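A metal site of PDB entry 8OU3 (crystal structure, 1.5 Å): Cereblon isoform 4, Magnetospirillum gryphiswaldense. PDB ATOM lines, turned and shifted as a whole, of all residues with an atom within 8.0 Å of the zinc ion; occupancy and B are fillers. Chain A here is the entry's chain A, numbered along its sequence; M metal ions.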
ATOM      1  N   ARG A  24     -25.072  -5.292 -22.763  1.00  0.00           N
ATOM      2  CA  ARG A  24     -25.290  -6.280 -23.828  1.00  0.00           C
ATOM      3  C   ARG A  24     -26.731  -6.176 -24.347  1.00  0.00           C
ATOM      4  O   ARG A  24     -27.550  -5.617 -23.658  1.00  0.00           O
ATOM      5  CB  ARG A  24     -25.095  -7.696 -23.265  1.00  0.00           C
ATOM      6  CG  ARG A  24     -23.676  -7.989 -22.809  1.00  0.00           C
ATOM      7  CD  ARG A  24     -23.535  -9.418 -22.298  1.00  0.00           C
ATOM      8  NE  ARG A  24     -22.157  -9.756 -21.987  1.00  0.00           N
ATOM      9  CZ  ARG A  24     -21.190  -9.858 -22.879  1.00  0.00           C
ATOM     10  NH1 ARG A  24     -21.467 -10.053 -24.155  1.00  0.00           N
ATOM     11  NH2 ARG A  24     -19.929  -9.754 -22.491  1.00  0.00           N
ATOM     12  N   CYS A  25     -26.982  -6.683 -25.563  1.00  0.00           N
ATOM     13  CA  CYS A  25     -28.329  -6.757 -26.092  1.00  0.00           C
ATOM     14  C   CYS A  25     -29.202  -7.617 -25.172  1.00  0.00           C
ATOM     15  O   CYS A  25     -28.805  -8.728 -24.825  1.00  0.00           O
ATOM     16  CB  CYS A  25     -28.291  -7.370 -27.484  1.00  0.00           C
ATOM     17  SG  CYS A  25     -29.950  -7.569 -28.177  1.00  0.00           S
ATOM     18  N   ARG A  26     -30.320  -7.079 -24.724  1.00  0.00           N
ATOM     19  CA  ARG A  26     -31.240  -7.797 -23.849  1.00  0.00           C
ATOM     20  C   ARG A  26     -31.771  -9.078 -24.482  1.00  0.00           C
ATOM     21  O   ARG A  26     -32.157 -10.009 -23.735  1.00  0.00           O
ATOM     22  CB  ARG A  26     -32.390  -6.837 -23.509  1.00  0.00           C
ATOM     23  CG  ARG A  26     -33.435  -7.409 -22.599  1.00  0.00           C
ATOM     24  CD  ARG A  26     -34.452  -6.342 -22.293  1.00  0.00           C
ATOM     25  NE  ARG A  26     -35.528  -6.975 -21.580  1.00  0.00           N
ATOM     26  CZ  ARG A  26     -36.633  -6.345 -21.147  1.00  0.00           C
ATOM     27  NH1 ARG A  26     -36.715  -5.016 -21.210  1.00  0.00           N
ATOM     28  NH2 ARG A  26     -37.599  -7.036 -20.565  1.00  0.00           N
ATOM     29  N   GLN A  27     -31.893  -9.107 -25.813  1.00  0.00           N
ATOM     30  CA  GLN A  27     -32.538 -10.259 -26.463  1.00  0.00           C
ATOM     31  C   GLN A  27     -31.565 -11.401 -26.695  1.00  0.00           C
ATOM     32  O   GLN A  27     -31.984 -12.552 -26.699  1.00  0.00           O
ATOM     33  CB  GLN A  27     -33.218  -9.850 -27.754  1.00  0.00           C
ATOM     34  CG  GLN A  27     -34.268  -8.782 -27.566  1.00  0.00           C
ATOM     35  CD  GLN A  27     -35.340  -9.135 -26.574  1.00  0.00           C
ATOM     36  OE1 GLN A  27     -35.791  -8.307 -25.789  1.00  0.00           O
ATOM     37  NE2 GLN A  27     -35.756 -10.380 -26.629  1.00  0.00           N
ATOM     38  N   CYS A  28     -30.272 -11.143 -26.842  1.00  0.00           N
ATOM     39  CA  CYS A  28     -29.355 -12.191 -27.266  1.00  0.00           C
ATOM     40  C   CYS A  28     -27.997 -12.178 -26.582  1.00  0.00           C
ATOM     41  O   CYS A  28     -27.194 -13.115 -26.733  1.00  0.00           O
ATOM     42  CB  CYS A  28     -29.170 -12.144 -28.775  1.00  0.00           C
ATOM     43  SG  CYS A  28     -28.109 -10.783 -29.312  1.00  0.00           S
ATOM     44  N   GLY A  29     -27.607 -11.104 -25.880  1.00  0.00           N
ATOM     45  CA  GLY A  29     -26.326 -11.120 -25.211  1.00  0.00           C
ATOM     46  C   GLY A  29     -25.141 -10.513 -25.963  1.00  0.00           C
ATOM     47  O   GLY A  29     -24.035 -10.424 -25.382  1.00  0.00           O
ATOM     48  N   GLN A  30     -25.319 -10.088 -27.215  1.00  0.00           N
ATOM     49  CA  GLN A  30     -24.241  -9.432 -27.949  1.00  0.00           C
ATOM     50  C   GLN A  30     -23.647  -8.301 -27.110  1.00  0.00           C
ATOM     51  O   GLN A  30     -24.392  -7.501 -26.546  1.00  0.00           O
ATOM     52  CB  GLN A  30     -24.826  -8.854 -29.241  1.00  0.00           C
ATOM     53  CG  GLN A  30     -23.863  -8.022 -30.078  1.00  0.00           C
ATOM     54  CD  GLN A  30     -23.020  -8.839 -31.006  1.00  0.00           C
ATOM     55  OE1 GLN A  30     -22.553  -9.906 -30.686  1.00  0.00           O
ATOM     56  NE2 GLN A  30     -22.961  -8.396 -32.244  1.00  0.00           N
ATOM     57  N   THR A  31     -22.308  -8.212 -27.077  1.00  0.00           N
ATOM     58  CA  THR A  31     -21.655  -7.087 -26.427  1.00  0.00           C
ATOM     59  C   THR A  31     -21.917  -5.788 -27.197  1.00  0.00           C
ATOM     60  O   THR A  31     -21.698  -5.800 -28.411  1.00  0.00           O
ATOM     61  CB  THR A  31     -20.133  -7.314 -26.356  1.00  0.00           C
ATOM     62  OG1 THR A  31     -19.871  -8.659 -25.969  1.00  0.00           O
ATOM     63  CG2 THR A  31     -19.518  -6.351 -25.384  1.00  0.00           C
ATOM     64  N   ILE A  32     -22.349  -4.707 -26.519  1.00  0.00           N
ATOM     65  CA  ILE A  32     -22.728  -3.483 -27.201  1.00  0.00           C
ATOM     66  C   ILE A  32     -21.908  -2.289 -26.680  1.00  0.00           C
ATOM     67  O   ILE A  32     -21.410  -1.500 -27.466  1.00  0.00           O
ATOM     68  CB  ILE A  32     -24.244  -3.179 -27.080  1.00  0.00           C
ATOM     69  CG1 ILE A  32     -25.129  -4.303 -27.623  1.00  0.00           C
ATOM     70  CG2 ILE A  32     -24.558  -1.861 -27.781  1.00  0.00           C
ATOM     71  CD1 ILE A  32     -24.941  -4.573 -29.112  1.00  0.00           C
ATOM     72  N   GLY A  67     -20.806  -4.116 -31.934  1.00  0.00           N
ATOM     73  CA  GLY A  67     -21.719  -5.226 -32.055  1.00  0.00           C
ATOM     74  C   GLY A  67     -23.047  -4.840 -32.704  1.00  0.00           C
ATOM     75  O   GLY A  67     -24.015  -5.617 -32.662  1.00  0.00           O
ATOM     76  N   LEU A  90     -29.130  -1.530 -35.374  1.00  0.00           N
ATOM     77  CA  LEU A  90     -29.658  -2.810 -34.922  1.00  0.00           C
ATOM     78  C   LEU A  90     -28.562  -3.578 -34.182  1.00  0.00           C
ATOM     79  O   LEU A  90     -27.389  -3.411 -34.446  1.00  0.00           O
ATOM     80  CB  LEU A  90     -30.135  -3.635 -36.118  1.00  0.00           C
ATOM     81  CG  LEU A  90     -31.135  -2.971 -37.073  1.00  0.00           C
ATOM     82  CD1 LEU A  90     -31.489  -3.940 -38.182  1.00  0.00           C
ATOM     83  CD2 LEU A  90     -32.352  -2.496 -36.311  1.00  0.00           C
ATOM     84  N   CYS A  91     -28.969  -4.461 -33.277  1.00  0.00           N
ATOM     85  CA  CYS A  91     -28.090  -5.486 -32.768  1.00  0.00           C
ATOM     86  C   CYS A  91     -27.566  -6.263 -33.971  1.00  0.00           C
ATOM     87  O   CYS A  91     -28.334  -6.775 -34.784  1.00  0.00           O
ATOM     88  CB  CYS A  91     -28.819  -6.486 -31.883  1.00  0.00           C
ATOM     89  SG  CYS A  91     -27.740  -7.781 -31.223  1.00  0.00           S
ATOM     90  N   GLY A  92     -26.216  -6.335 -34.118  1.00  0.00           N
ATOM     91  CA  GLY A  92     -25.651  -7.022 -35.261  1.00  0.00           C
ATOM     92  C   GLY A  92     -25.811  -8.533 -35.227  1.00  0.00           C
ATOM     93  O   GLY A  92     -25.645  -9.186 -36.269  1.00  0.00           O
ATOM     94  N   GLN A  93     -26.188  -9.090 -34.066  1.00  0.00           N
ATOM     95  CA  GLN A  93     -26.397 -10.495 -33.878  1.00  0.00           C
ATOM     96  C   GLN A  93     -27.864 -10.827 -34.163  1.00  0.00           C
ATOM     97  O   GLN A  93     -28.126 -11.644 -35.025  1.00  0.00           O
ATOM     98  CB  GLN A  93     -25.867 -10.944 -32.524  1.00  0.00           C
ATOM     99  CG  GLN A  93     -26.043 -12.387 -32.211  1.00  0.00           C
ATOM    100  CD  GLN A  93     -25.111 -12.812 -31.092  1.00  0.00           C
ATOM    101  OE1 GLN A  93     -24.011 -13.302 -31.339  1.00  0.00           O
ATOM    102  NE2 GLN A  93     -25.506 -12.624 -29.855  1.00  0.00           N
ATOM    103  N   CYS A  94     -28.818 -10.228 -33.440  1.00  0.00           N
ATOM    104  CA  CYS A  94     -30.203 -10.668 -33.527  1.00  0.00           C
ATOM    105  C   CYS A  94     -31.152  -9.723 -34.265  1.00  0.00           C
ATOM    106  O   CYS A  94     -32.279 -10.132 -34.525  1.00  0.00           O
ATOM    107  CB  CYS A  94     -30.775 -10.930 -32.155  1.00  0.00           C
ATOM    108  SG  CYS A  94     -31.236  -9.460 -31.195  1.00  0.00           S
ATOM    109  N   GLY A  95     -30.687  -8.517 -34.606  1.00  0.00           N
ATOM    110  CA  GLY A  95     -31.523  -7.604 -35.361  1.00  0.00           C
ATOM    111  C   GLY A  95     -32.456  -6.723 -34.509  1.00  0.00           C
ATOM    112  O   GLY A  95     -33.131  -5.871 -35.081  1.00  0.00           O
ATOM    113  N   SER A  96     -32.418  -6.873 -33.207  1.00  0.00           N
ATOM    114  CA  SER A  96     -33.183  -6.010 -32.293  1.00  0.00           C
ATOM    115  C   SER A  96     -32.818  -4.549 -32.545  1.00  0.00           C
ATOM    116  O   SER A  96     -31.657  -4.205 -32.700  1.00  0.00           O
ATOM    117  CB  SER A  96     -32.888  -6.347 -30.853  1.00  0.00           C
ATOM    118  OG  SER A  96     -33.673  -5.526 -29.958  1.00  0.00           O
ATOM    119  N   HIS A  97     -33.823  -3.666 -32.603  1.00  0.00           N
ATOM    120  CA  HIS A  97     -33.521  -2.255 -32.793  1.00  0.00           C
ATOM    121  C   HIS A  97     -33.058  -1.622 -31.475  1.00  0.00           C
ATOM    122  O   HIS A  97     -33.855  -1.478 -30.535  1.00  0.00           O
ATOM    123  CB  HIS A  97     -34.739  -1.501 -33.308  1.00  0.00           C
ATOM    124  CG  HIS A  97     -34.526  -0.046 -33.404  1.00  0.00           C
ATOM    125  ND1 HIS A  97     -35.571   0.872 -33.323  1.00  0.00           N
ATOM    126  CD2 HIS A  97     -33.408   0.658 -33.652  1.00  0.00           C
ATOM    127  CE1 HIS A  97     -35.070   2.083 -33.483  1.00  0.00           C
ATOM    128  NE2 HIS A  97     -33.757   1.980 -33.690  1.00  0.00           N
ATOM    129  N   LEU A  98     -31.735  -1.380 -31.341  1.00  0.00           N
ATOM    130  CA  LEU A  98     -31.177  -0.908 -30.090  1.00  0.00           C
ATOM    131  C   LEU A  98     -31.044   0.597 -29.972  1.00  0.00           C
ATOM    132  O   LEU A  98     -30.890   1.115 -28.868  1.00  0.00           O
ATOM    133  CB  LEU A  98     -29.823  -1.575 -29.864  1.00  0.00           C
ATOM    134  CG  LEU A  98     -29.875  -3.095 -29.705  1.00  0.00           C
ATOM    135  CD1 LEU A  98     -28.490  -3.590 -29.261  1.00  0.00           C
ATOM    136  CD2 LEU A  98     -30.925  -3.596 -28.723  1.00  0.00           C
ATOM    137  N   ARG A 118     -33.614  -1.761 -23.720  1.00  0.00           N
ATOM    138  CA  ARG A 118     -33.299  -2.816 -24.679  1.00  0.00           C
ATOM    139  C   ARG A 118     -31.906  -3.412 -24.470  1.00  0.00           C
ATOM    140  O   ARG A 118     -31.424  -4.238 -25.265  1.00  0.00           O
ATOM    141  CB  ARG A 118     -33.523  -2.253 -26.082  1.00  0.00           C
ATOM    142  CG  ARG A 118     -34.972  -1.858 -26.308  1.00  0.00           C
ATOM    143  CD  ARG A 118     -35.300  -1.553 -27.753  1.00  0.00           C
ATOM    144  NE  ARG A 118     -36.633  -0.987 -27.853  1.00  0.00           N
ATOM    145  CZ  ARG A 118     -37.245  -0.615 -28.973  1.00  0.00           C
ATOM    146  NH1 ARG A 118     -36.658  -0.859 -30.137  1.00  0.00           N
ATOM    147  NH2 ARG A 118     -38.482  -0.115 -28.927  1.00  0.00           N
HETATM  148 ZN    ZN M   1     -29.363  -8.899 -29.944  1.00  0.00          ZN
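Four residues have an atom within 4 Å of the zinc ion: Cys 25, Cys 28, Cys 91 and Cys 94.
The side-chain sulfur (SG) of Cys 25 sits close to the backbone NH (N) of Gln 27 (3.4 Å).
The backbone NH (N) of Cys 25 sits at hydrogen-bond distance from the backbone carbonyl oxygen (O) of Gln 30, 2.9 Å away.
The side-chain sulfur of Cys 94 lies close to the backbone NH of Ser 96 (3.5 Å).
The backbone NH of Cys 91 lies within hydrogen-bond range of the backbone carbonyl oxygen of Ser 96 (2.8 Å).
SG of Cys 91 sits close to N of Gln 93 (3.5 Å).
The backbone NH (N) of Gln 30 sits close to the side-chain sulfur (SG) of Cys 28 (3.6 Å).
NE2 of Gln 93 lies close to SG of Cys 28, 3.2 Å away.
The zinc ion is bound by SG of Cys 25 (2.3 Å), SG of Cys 94 (2.3 Å), SG of Cys 91 (2.3 Å) and SG of Cys 28 (2.3 Å).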
